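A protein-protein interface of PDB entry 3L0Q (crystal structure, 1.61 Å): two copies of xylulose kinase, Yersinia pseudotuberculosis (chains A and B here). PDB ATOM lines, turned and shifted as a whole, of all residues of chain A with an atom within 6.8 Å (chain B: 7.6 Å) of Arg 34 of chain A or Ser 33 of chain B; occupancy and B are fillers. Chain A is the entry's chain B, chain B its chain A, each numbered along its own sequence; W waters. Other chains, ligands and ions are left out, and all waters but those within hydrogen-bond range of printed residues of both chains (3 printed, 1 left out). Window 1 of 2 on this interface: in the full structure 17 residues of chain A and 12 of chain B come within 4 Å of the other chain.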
ATOM      1  N   GLY A  15      14.842 -28.016  36.962  1.00  0.00           N
ATOM      2  CA  GLY A  15      14.202 -27.110  36.034  1.00  0.00           C
ATOM      3  C   GLY A  15      13.947 -27.656  34.642  1.00  0.00           C
ATOM      4  O   GLY A  15      13.089 -27.143  33.934  1.00  0.00           O
ATOM      5  N   SER A  16      14.696 -28.651  34.224  1.00  0.00           N
ATOM      6  CA  SER A  16      14.570 -29.154  32.858  1.00  0.00           C
ATOM      7  C   SER A  16      14.862 -30.619  32.720  1.00  0.00           C
ATOM      8  O   SER A  16      15.562 -31.158  33.492  1.00  0.00           O
ATOM      9  CB  SER A  16      15.594 -28.479  31.965  1.00  0.00           C
ATOM     10  OG  SER A  16      15.334 -27.147  31.835  1.00  0.00           O
ATOM     11  N   ALA A  17      14.372 -31.195  31.649  1.00  0.00           N
ATOM     12  CA  ALA A  17      14.757 -32.485  31.204  1.00  0.00           C
ATOM     13  C   ALA A  17      15.694 -32.318  30.043  1.00  0.00           C
ATOM     14  O   ALA A  17      15.427 -31.589  29.152  1.00  0.00           O
ATOM     15  CB  ALA A  17      13.572 -33.277  30.774  1.00  0.00           C
ATOM     16  N   ARG A  18      16.812 -32.989  30.125  1.00  0.00           N
ATOM     17  CA  ARG A  18      17.847 -32.907  29.135  1.00  0.00           C
ATOM     18  C   ARG A  18      18.231 -34.260  28.584  1.00  0.00           C
ATOM     19  O   ARG A  18      18.221 -35.224  29.252  1.00  0.00           O
ATOM     20  CB  ARG A  18      19.094 -32.214  29.702  1.00  0.00           C
ATOM     21  CG  ARG A  18      18.863 -30.817  30.106  1.00  0.00           C
ATOM     22  CD  ARG A  18      20.151 -30.084  30.522  1.00  0.00           C
ATOM     23  NE  ARG A  18      20.836 -30.832  31.503  1.00  0.00           N
ATOM     24  CZ  ARG A  18      22.119 -31.137  31.487  1.00  0.00           C
ATOM     25  NH1 ARG A  18      22.575 -31.928  32.417  1.00  0.00           N
ATOM     26  NH2 ARG A  18      22.926 -30.663  30.562  1.00  0.00           N
ATOM     27  N   ALA A  19      18.584 -34.268  27.312  1.00  0.00           N
ATOM     28  CA  ALA A  19      19.046 -35.470  26.678  1.00  0.00           C
ATOM     29  C   ALA A  19      20.305 -35.219  25.881  1.00  0.00           C
ATOM     30  O   ALA A  19      20.450 -34.211  25.259  1.00  0.00           O
ATOM     31  CB  ALA A  19      17.987 -36.086  25.785  1.00  0.00           C
ATOM     32  N   ALA A  32      19.578 -31.680  23.643  1.00  0.00           N
ATOM     33  CA  ALA A  32      18.361 -30.836  23.667  1.00  0.00           C
ATOM     34  C   ALA A  32      17.782 -30.822  25.076  1.00  0.00           C
ATOM     35  O   ALA A  32      18.176 -31.654  25.903  1.00  0.00           O
ATOM     36  CB  ALA A  32      17.311 -31.327  22.632  1.00  0.00           C
ATOM     37  N   SER A  33      16.848 -29.888  25.336  1.00  0.00           N
ATOM     38  CA  SER A  33      16.385 -29.560  26.673  1.00  0.00           C
ATOM     39  C   SER A  33      14.914 -29.195  26.554  1.00  0.00           C
ATOM     40  O   SER A  33      14.496 -28.637  25.529  1.00  0.00           O
ATOM     41  CB  SER A  33      17.136 -28.321  27.153  1.00  0.00           C
ATOM     42  OG  SER A  33      17.656 -28.511  28.452  1.00  0.00           O
ATOM     43  N   ARG A  34      14.146 -29.505  27.593  1.00  0.00           N
ATOM     44  CA  ARG A  34      12.775 -28.976  27.740  1.00  0.00           C
ATOM     45  C   ARG A  34      12.519 -28.609  29.187  1.00  0.00           C
ATOM     46  O   ARG A  34      12.760 -29.418  30.089  1.00  0.00           O
ATOM     47  CB  ARG A  34      11.749 -30.019  27.266  1.00  0.00           C
ATOM     48  CG  ARG A  34      11.664 -30.183  25.743  1.00  0.00           C
ATOM     49  CD  ARG A  34      11.272 -28.866  25.069  1.00  0.00           C
ATOM     50  NE  ARG A  34      10.869 -29.141  23.692  1.00  0.00           N
ATOM     51  CZ  ARG A  34      11.717 -29.410  22.699  1.00  0.00           C
ATOM     52  NH1 ARG A  34      13.020 -29.419  22.920  1.00  0.00           N
ATOM     53  NH2 ARG A  34      11.257 -29.651  21.471  1.00  0.00           N
ATOM     54  N   GLU A  35      12.017 -27.410  29.447  1.00  0.00           N
ATOM     55  CA  GLU A  35      11.721 -27.025  30.819  1.00  0.00           C
ATOM     56  C   GLU A  35      10.568 -27.853  31.357  1.00  0.00           C
ATOM     57  O   GLU A  35       9.696 -28.292  30.594  1.00  0.00           O
ATOM     58  CB  GLU A  35      11.398 -25.533  30.860  1.00  0.00           C
ATOM     59  CG  GLU A  35      12.608 -24.694  30.518  1.00  0.00           C
ATOM     60  CD  GLU A  35      12.943 -24.674  29.016  1.00  0.00           C
ATOM     61  OE1 GLU A  35      12.032 -24.767  28.163  1.00  0.00           O
ATOM     62  OE2 GLU A  35      14.156 -24.579  28.698  1.00  0.00           O
ATOM     63  N   ILE A  36      10.582 -28.110  32.663  1.00  0.00           N
ATOM     64  CA  ILE A  36       9.474 -28.844  33.277  1.00  0.00           C
ATOM     65  C   ILE A  36       8.842 -27.936  34.293  1.00  0.00           C
ATOM     66  O   ILE A  36       9.503 -27.052  34.863  1.00  0.00           O
ATOM     67  CB  ILE A  36       9.939 -30.218  33.875  1.00  0.00           C
ATOM     68  CG1 ILE A  36      11.038 -30.025  34.890  1.00  0.00           C
ATOM     69  CG2 ILE A  36      10.441 -31.166  32.760  1.00  0.00           C
ATOM     70  CD1 ILE A  36      11.417 -31.303  35.652  1.00  0.00           C
ATOM     71  N   GLN A  55       6.719 -36.075  28.994  1.00  0.00           N
ATOM     72  CA  GLN A  55       6.600 -35.354  27.711  1.00  0.00           C
ATOM     73  C   GLN A  55       7.889 -34.553  27.410  1.00  0.00           C
ATOM     74  O   GLN A  55       8.394 -34.574  26.286  1.00  0.00           O
ATOM     75  CB  GLN A  55       5.406 -34.412  27.676  1.00  0.00           C
ATOM     76  CG  GLN A  55       5.534 -33.535  26.456  1.00  0.00           C
ATOM     77  CD  GLN A  55       4.226 -32.995  25.955  1.00  0.00           C
ATOM     78  OE1 GLN A  55       3.179 -33.122  26.631  1.00  0.00           O
ATOM     79  NE2 GLN A  55       4.260 -32.375  24.745  1.00  0.00           N
ATOM     80  N   ALA A  56       8.425 -33.894  28.443  1.00  0.00           N
ATOM     81  CA  ALA A  56       9.674 -33.146  28.316  1.00  0.00           C
ATOM     82  C   ALA A  56      10.821 -34.055  27.903  1.00  0.00           C
ATOM     83  O   ALA A  56      11.570 -33.737  26.994  1.00  0.00           O
ATOM     84  CB  ALA A  56      10.006 -32.341  29.610  1.00  0.00           C
ATOM     85  N   VAL A  57      10.977 -35.190  28.591  1.00  0.00           N
ATOM     86  CA  VAL A  57      11.967 -36.175  28.224  1.00  0.00           C
ATOM     87  C   VAL A  57      11.809 -36.642  26.759  1.00  0.00           C
ATOM     88  O   VAL A  57      12.794 -36.723  26.015  1.00  0.00           O
ATOM     89  CB  VAL A  57      11.865 -37.434  29.139  1.00  0.00           C
ATOM     90  CG1 VAL A  57      12.643 -38.593  28.541  1.00  0.00           C
ATOM     91  CG2 VAL A  57      12.335 -37.148  30.575  1.00  0.00           C
ATOM     92  N   CYS A  58      10.595 -36.977  26.330  1.00  0.00           N
ATOM     93  CA  CYS A  58      10.419 -37.476  24.955  1.00  0.00           C
ATOM     94  C   CYS A  58      10.752 -36.404  23.907  1.00  0.00           C
ATOM     95  O   CYS A  58      11.384 -36.709  22.898  1.00  0.00           O
ATOM     96  CB  CYS A  58       8.998 -38.002  24.732  1.00  0.00           C
ATOM     97  SG  CYS A  58       8.654 -39.474  25.720  1.00  0.00           S
ATOM     98  N   ASN A  59      10.340 -35.158  24.142  1.00  0.00           N
ATOM     99  CA  ASN A  59      10.652 -34.083  23.214  1.00  0.00           C
ATOM    100  C   ASN A  59      12.161 -33.834  23.185  1.00  0.00           C
ATOM    101  O   ASN A  59      12.747 -33.636  22.110  1.00  0.00           O
ATOM    102  CB  ASN A  59       9.910 -32.797  23.575  1.00  0.00           C
ATOM    103  CG  ASN A  59       8.465 -32.858  23.179  1.00  0.00           C
ATOM    104  OD1 ASN A  59       8.109 -33.497  22.178  1.00  0.00           O
ATOM    105  ND2 ASN A  59       7.618 -32.227  23.961  1.00  0.00           N
ATOM    106  N   ALA A  60      12.786 -33.840  24.367  1.00  0.00           N
ATOM    107  CA  ALA A  60      14.232 -33.604  24.432  1.00  0.00           C
ATOM    108  C   ALA A  60      14.981 -34.698  23.675  1.00  0.00           C
ATOM    109  O   ALA A  60      15.957 -34.410  22.948  1.00  0.00           O
ATOM    110  CB  ALA A  60      14.726 -33.541  25.929  1.00  0.00           C
ATOM    111  N   VAL A  61      14.580 -35.960  23.885  1.00  0.00           N
ATOM    112  CA  VAL A  61      15.225 -37.060  23.212  1.00  0.00           C
ATOM    113  C   VAL A  61      15.016 -36.951  21.702  1.00  0.00           C
ATOM    114  O   VAL A  61      15.974 -37.150  20.944  1.00  0.00           O
ATOM    115  CB  VAL A  61      14.692 -38.429  23.698  1.00  0.00           C
ATOM    116  CG1 VAL A  61      15.117 -39.597  22.759  1.00  0.00           C
ATOM    117  CG2 VAL A  61      15.232 -38.674  25.095  1.00  0.00           C
ATOM    118  N   ASP A  63      14.561 -34.255  19.907  1.00  0.00           N
ATOM    119  CA  ASP A  63      15.359 -33.151  19.371  1.00  0.00           C
ATOM    120  C   ASP A  63      16.849 -33.463  19.390  1.00  0.00           C
ATOM    121  O   ASP A  63      17.583 -33.047  18.503  1.00  0.00           O
ATOM    122  CB  ASP A  63      15.114 -31.838  20.118  1.00  0.00           C
ATOM    123  CG  ASP A  63      13.808 -31.205  19.750  1.00  0.00           C
ATOM    124  OD1 ASP A  63      13.082 -31.843  18.945  1.00  0.00           O
ATOM    125  OD2 ASP A  63      13.550 -30.052  20.226  1.00  0.00           O
ATOM    126  N   ASP B  11      10.469 -17.513  14.976  1.00  0.00           N
ATOM    127  CA  ASP B  11       9.235 -17.806  14.260  1.00  0.00           C
ATOM    128  C   ASP B  11       8.262 -18.539  15.175  1.00  0.00           C
ATOM    129  O   ASP B  11       8.523 -19.682  15.611  1.00  0.00           O
ATOM    130  CB  ASP B  11       9.582 -18.693  13.043  1.00  0.00           C
ATOM    131  CG  ASP B  11       8.378 -19.413  12.461  1.00  0.00           C
ATOM    132  OD1 ASP B  11       7.344 -18.797  12.156  1.00  0.00           O
ATOM    133  OD2 ASP B  11       8.493 -20.644  12.252  1.00  0.00           O
ATOM    134  N   GLY B  15       2.209 -24.644  16.294  1.00  0.00           N
ATOM    135  CA  GLY B  15       2.520 -25.640  17.315  1.00  0.00           C
ATOM    136  C   GLY B  15       3.708 -25.355  18.188  1.00  0.00           C
ATOM    137  O   GLY B  15       3.724 -25.844  19.309  1.00  0.00           O
ATOM    138  N   SER B  16       4.685 -24.572  17.692  1.00  0.00           N
ATOM    139  CA  SER B  16       5.953 -24.348  18.403  1.00  0.00           C
ATOM    140  C   SER B  16       6.496 -22.954  18.110  1.00  0.00           C
ATOM    141  O   SER B  16       6.203 -22.386  17.052  1.00  0.00           O
ATOM    142  CB  SER B  16       7.040 -25.355  17.989  1.00  0.00           C
ATOM    143  OG  SER B  16       6.657 -26.696  18.286  1.00  0.00           O
ATOM    144  N   ALA B  17       7.290 -22.450  19.049  1.00  0.00           N
ATOM    145  CA  ALA B  17       8.123 -21.282  18.823  1.00  0.00           C
ATOM    146  C   ALA B  17       9.520 -21.850  18.441  1.00  0.00           C
ATOM    147  O   ALA B  17      10.093 -22.712  19.146  1.00  0.00           O
ATOM    148  CB  ALA B  17       8.203 -20.475  20.053  1.00  0.00           C
ATOM    149  N   ARG B  18      10.083 -21.365  17.346  1.00  0.00           N
ATOM    150  CA  ARG B  18      11.414 -21.799  16.911  1.00  0.00           C
ATOM    151  C   ARG B  18      12.325 -20.578  16.874  1.00  0.00           C
ATOM    152  O   ARG B  18      11.857 -19.457  16.707  1.00  0.00           O
ATOM    153  CB  ARG B  18      11.379 -22.388  15.507  1.00  0.00           C
ATOM    154  CG  ARG B  18      10.578 -23.676  15.336  1.00  0.00           C
ATOM    155  CD  ARG B  18      10.456 -23.947  13.860  1.00  0.00           C
ATOM    156  NE  ARG B  18       9.267 -23.249  13.404  1.00  0.00           N
ATOM    157  CZ  ARG B  18       8.040 -23.698  13.661  1.00  0.00           C
ATOM    158  NH1 ARG B  18       7.904 -24.840  14.345  1.00  0.00           N
ATOM    159  NH2 ARG B  18       6.957 -23.027  13.241  1.00  0.00           N
ATOM    160  N   ALA B  19      13.628 -20.793  17.043  1.00  0.00           N
ATOM    161  CA  ALA B  19      14.603 -19.698  16.931  1.00  0.00           C
ATOM    162  C   ALA B  19      15.768 -20.215  16.102  1.00  0.00           C
ATOM    163  O   ALA B  19      16.147 -21.379  16.243  1.00  0.00           O
ATOM    164  CB  ALA B  19      15.103 -19.190  18.339  1.00  0.00           C
ATOM    165  N   GLN B  31      19.886 -23.730  16.163  1.00  0.00           N
ATOM    166  CA  GLN B  31      18.429 -23.617  16.208  1.00  0.00           C
ATOM    167  C   GLN B  31      17.880 -24.384  17.390  1.00  0.00           C
ATOM    168  O   GLN B  31      18.520 -25.347  17.890  1.00  0.00           O
ATOM    169  CB  GLN B  31      17.828 -24.130  14.913  1.00  0.00           C
ATOM    170  CG  GLN B  31      17.983 -25.574  14.687  1.00  0.00           C
ATOM    171  CD  GLN B  31      17.244 -26.030  13.447  1.00  0.00           C
ATOM    172  OE1 GLN B  31      16.250 -25.400  13.037  1.00  0.00           O
ATOM    173  NE2 GLN B  31      17.715 -27.115  12.838  1.00  0.00           N
ATOM    174  N   ALA B  32      16.687 -23.987  17.835  1.00  0.00           N
ATOM    175  CA  ALA B  32      15.988 -24.739  18.866  1.00  0.00           C
ATOM    176  C   ALA B  32      14.488 -24.501  18.706  1.00  0.00           C
ATOM    177  O   ALA B  32      14.104 -23.625  17.953  1.00  0.00           O
ATOM    178  CB  ALA B  32      16.427 -24.293  20.207  1.00  0.00           C
ATOM    179  N   SER B  33      13.674 -25.302  19.393  1.00  0.00           N
ATOM    180  CA  SER B  33      12.212 -25.185  19.310  1.00  0.00           C
ATOM    181  C   SER B  33      11.600 -25.450  20.679  1.00  0.00           C
ATOM    182  O   SER B  33      12.168 -26.185  21.491  1.00  0.00           O
ATOM    183  CB  SER B  33      11.743 -26.260  18.320  1.00  0.00           C
ATOM    184  OG  SER B  33      10.383 -26.115  17.986  1.00  0.00           O
ATOM    185  N   ARG B  34      10.406 -24.902  20.927  1.00  0.00           N
ATOM    186  CA  ARG B  34       9.678 -25.199  22.154  1.00  0.00           C
ATOM    187  C   ARG B  34       8.183 -25.268  21.784  1.00  0.00           C
ATOM    188  O   ARG B  34       7.667 -24.335  21.190  1.00  0.00           O
ATOM    189  CB  ARG B  34       9.867 -24.085  23.186  1.00  0.00           C
ATOM    190  CG  ARG B  34      11.257 -24.068  23.816  1.00  0.00           C
ATOM    191  CD  ARG B  34      11.510 -25.400  24.572  1.00  0.00           C
ATOM    192  NE  ARG B  34      12.668 -25.259  25.459  1.00  0.00           N
ATOM    193  CZ  ARG B  34      13.923 -25.496  25.064  1.00  0.00           C
ATOM    194  NH1 ARG B  34      14.142 -25.872  23.823  1.00  0.00           N
ATOM    195  NH2 ARG B  34      14.928 -25.368  25.914  1.00  0.00           N
ATOM    196  N   GLU B  35       7.500 -26.349  22.146  1.00  0.00           N
ATOM    197  CA  GLU B  35       6.046 -26.405  21.991  1.00  0.00           C
ATOM    198  C   GLU B  35       5.255 -25.307  22.676  1.00  0.00           C
ATOM    199  O   GLU B  35       5.595 -24.808  23.769  1.00  0.00           O
ATOM    200  CB  GLU B  35       5.541 -27.760  22.492  1.00  0.00           C
ATOM    201  CG  GLU B  35       6.123 -28.895  21.713  1.00  0.00           C
ATOM    202  CD  GLU B  35       7.572 -29.258  22.084  1.00  0.00           C
ATOM    203  OE1 GLU B  35       8.055 -28.923  23.194  1.00  0.00           O
ATOM    204  OE2 GLU B  35       8.197 -29.883  21.220  1.00  0.00           O
ATOM    205  N   ILE B  36       4.195 -24.887  22.022  1.00  0.00           N
ATOM    206  CA  ILE B  36       3.286 -23.942  22.658  1.00  0.00           C
ATOM    207  C   ILE B  36       1.909 -24.589  22.859  1.00  0.00           C
ATOM    208  O   ILE B  36       1.442 -25.360  22.020  1.00  0.00           O
ATOM    209  CB  ILE B  36       3.212 -22.583  21.936  1.00  0.00           C
ATOM    210  CG1 ILE B  36       2.812 -22.724  20.476  1.00  0.00           C
ATOM    211  CG2 ILE B  36       4.544 -21.799  22.095  1.00  0.00           C
ATOM    212  CD1 ILE B  36       2.564 -21.323  19.832  1.00  0.00           C
ATOM    213  N   ALA B  56       8.247 -19.806  25.715  1.00  0.00           N
ATOM    214  CA  ALA B  56       8.771 -20.689  24.694  1.00  0.00           C
ATOM    215  C   ALA B  56       9.774 -19.973  23.806  1.00  0.00           C
ATOM    216  O   ALA B  56      10.807 -20.541  23.461  1.00  0.00           O
ATOM    217  CB  ALA B  56       7.628 -21.260  23.860  1.00  0.00           C
ATOM    218  N   VAL B  57       9.437 -18.765  23.378  1.00  0.00           N
ATOM    219  CA  VAL B  57      10.339 -17.950  22.575  1.00  0.00           C
ATOM    220  C   VAL B  57      11.685 -17.745  23.265  1.00  0.00           C
ATOM    221  O   VAL B  57      12.727 -18.001  22.668  1.00  0.00           O
ATOM    222  CB  VAL B  57       9.726 -16.585  22.248  1.00  0.00           C
ATOM    223  CG1 VAL B  57      10.814 -15.625  21.783  1.00  0.00           C
ATOM    224  CG2 VAL B  57       8.633 -16.743  21.172  1.00  0.00           C
ATOM    225  N   ASN B  59      13.065 -19.395  25.836  1.00  0.00           N
ATOM    226  CA  ASN B  59      13.810 -20.630  25.982  1.00  0.00           C
ATOM    227  C   ASN B  59      14.393 -21.122  24.670  1.00  0.00           C
ATOM    228  O   ASN B  59      15.562 -21.523  24.636  1.00  0.00           O
ATOM    229  CB  ASN B  59      12.938 -21.698  26.625  1.00  0.00           C
ATOM    230  CG  ASN B  59      12.704 -21.413  28.088  1.00  0.00           C
ATOM    231  OD1 ASN B  59      11.622 -21.649  28.620  1.00  0.00           O
ATOM    232  ND2 ASN B  59      13.722 -20.859  28.736  1.00  0.00           N
ATOM    233  N   ALA B  60      13.600 -21.028  23.588  1.00  0.00           N
ATOM    234  CA  ALA B  60      14.099 -21.350  22.258  1.00  0.00           C
ATOM    235  C   ALA B  60      15.310 -20.503  21.859  1.00  0.00           C
ATOM    236  O   ALA B  60      16.270 -21.008  21.253  1.00  0.00           O
ATOM    237  CB  ALA B  60      13.002 -21.202  21.203  1.00  0.00           C
ATOM    238  N   VAL B  61      15.249 -19.204  22.157  1.00  0.00           N
ATOM    239  CA  VAL B  61      16.341 -18.327  21.785  1.00  0.00           C
ATOM    240  C   VAL B  61      17.600 -18.721  22.588  1.00  0.00           C
ATOM    241  O   VAL B  61      18.667 -18.864  22.028  1.00  0.00           O
ATOM    242  CB  VAL B  61      15.989 -16.881  21.958  1.00  0.00           C
ATOM    243  CG1 VAL B  61      17.238 -16.019  21.953  1.00  0.00           C
ATOM    244  CG2 VAL B  61      15.078 -16.454  20.781  1.00  0.00           C
ATOM    245  N   ASP B  63      18.537 -21.474  23.844  1.00  0.00           N
ATOM    246  CA  ASP B  63      18.994 -22.784  23.416  1.00  0.00           C
ATOM    247  C   ASP B  63      19.680 -22.691  22.071  1.00  0.00           C
ATOM    248  O   ASP B  63      20.691 -23.339  21.865  1.00  0.00           O
ATOM    249  CB  ASP B  63      17.767 -23.701  23.323  1.00  0.00           C
ATOM    250  CG  ASP B  63      18.096 -25.191  23.192  1.00  0.00           C
ATOM    251  OD1 ASP B  63      19.241 -25.586  22.863  1.00  0.00           O
ATOM    252  OD2 ASP B  63      17.150 -26.001  23.361  1.00  0.00           O
ATOM    253  N   ALA B  64      19.088 -21.924  21.140  1.00  0.00           N
ATOM    254  CA  ALA B  64      19.644 -21.758  19.798  1.00  0.00           C
ATOM    255  C   ALA B  64      21.026 -21.098  19.828  1.00  0.00           C
ATOM    256  O   ALA B  64      21.938 -21.510  19.100  1.00  0.00           O
ATOM    257  CB  ALA B  64      18.701 -20.944  18.925  1.00  0.00           C
HETATM  258  O   HOH W   1      15.098 -27.872  20.369  1.00  0.00           O
HETATM  259  O   HOH W   2      16.555 -22.669  27.241  1.00  0.00           O
HETATM  260  O   HOH W   3       9.601 -22.980  26.998  1.00  0.00           O
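The backbone carbonyl oxygen (O) of Ser 33 of chain A sits close to the guanidinium group (NH1) of Arg 34 of chain B (3.3 Å).
The guanidinium group of Arg 34 of chain B lies within salt-bridge range of the side-chain carboxylate of Glu 35 of chain A (2.8 Å).
The side-chain carboxylate (OE1) of Glu 35 of chain B lies within salt-bridge range of the guanidinium group (NE) of Arg 34 of chain A (2.9 Å).
The side-chain carboxylate of Glu 35 of chain B lies within hydrogen-bond range of the side-chain amide nitrogen of Asn 59 of chain A (3.4 Å).
OD1 of Asn 59 of chain B lies close to OE1 of Glu 35 of chain A, 3.2 Å away.
Ser 33 of chain A touches Arg 34 of chain B, and with the chains exchanged Arg 34 of chain A touches Ser 33 of chain B.
Arg 34 of chain B touches its own counterpart, Arg 34 of chain A.
Arg 34 of chain A touches Glu 35 of chain B, and with the chains exchanged Glu 35 of chain A touches Arg 34 of chain B.
Glu 35 of chain A touches Asn 59 of chain B, and with the chains exchanged Asn 59 of chain A touches Glu 35 of chain B.
Of the 7 pairs that touch across the chains among the printed residues, 7 have their exchanged pair printed and touching as well.
Water W1 lies within hydrogen-bond range of OD2 of Asp 63 of chain A (2.7 Å) and N of Ser 33 of chain B (3.1 Å).
Water W3 bridges the side-chain amide oxygen (OD1) of Asn 59 of chain B and the side-chain carboxylate (OE1) of Glu 35 of chain A.
Water W2 lies within hydrogen-bond range of O of Asn 59 of chain B (3.0 Å), OE2 of Glu 35 of chain A (3.4 Å) and NH2 of Arg 34 of chain B (3.4 Å).
Among the printed residues, pairs that only touch across the chains: Arg 34 of chain A with Ser 33 of chain B and Arg 34 of chain A with Arg 34 of chain B.
N of Arg 34 of chain B lies within hydrogen-bond range of O of Ala 17 of chain B (2.8 Å).
OD2 of Asp 63 of chain B lies within salt-bridge range of NH1 of Arg 34 of chain B, at 3.0 Å.
The backbone NH (N) of Ala 17 of chain A lies within hydrogen-bond range of the backbone carbonyl oxygen (O) of Arg 34 of chain A (2.9 Å).
OD2 of Asp 63 of chain A is in salt-bridge range of NH2 of Arg 34 of chain A, at 2.6 Å.
The backbone carbonyl oxygen of Gln 55 of chain A lies within hydrogen-bond range of the side-chain amide nitrogen of Asn 59 of chain A, at 3.4 Å.
Printed residues of chain A that touch a printed residue of chain B: Ser 33, Arg 34, Glu 35 and Asn 59.
Among the printed residues, 7 pairs touch across the chains.
Of the printed residues of chain B, Arg 34 of chain A touches Ser 33, Arg 34 and Glu 35.
Ser 33 of chain B touches just one residue of chain A: Arg 34.
Of the printed residues of chain B, Asn 59 of chain A touches Glu 35.
Of the printed residues of chain A, Asn 59 of chain B touches Glu 35.
Ala 17 of chain B touches none of the printed residues of chain A.
Ala 19 of chain A touches none of the printed residues of chain B.
The nearest residue of chain A that does not touch Ser 33 of chain B is Asp 63 of chain A (4.3 Å).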
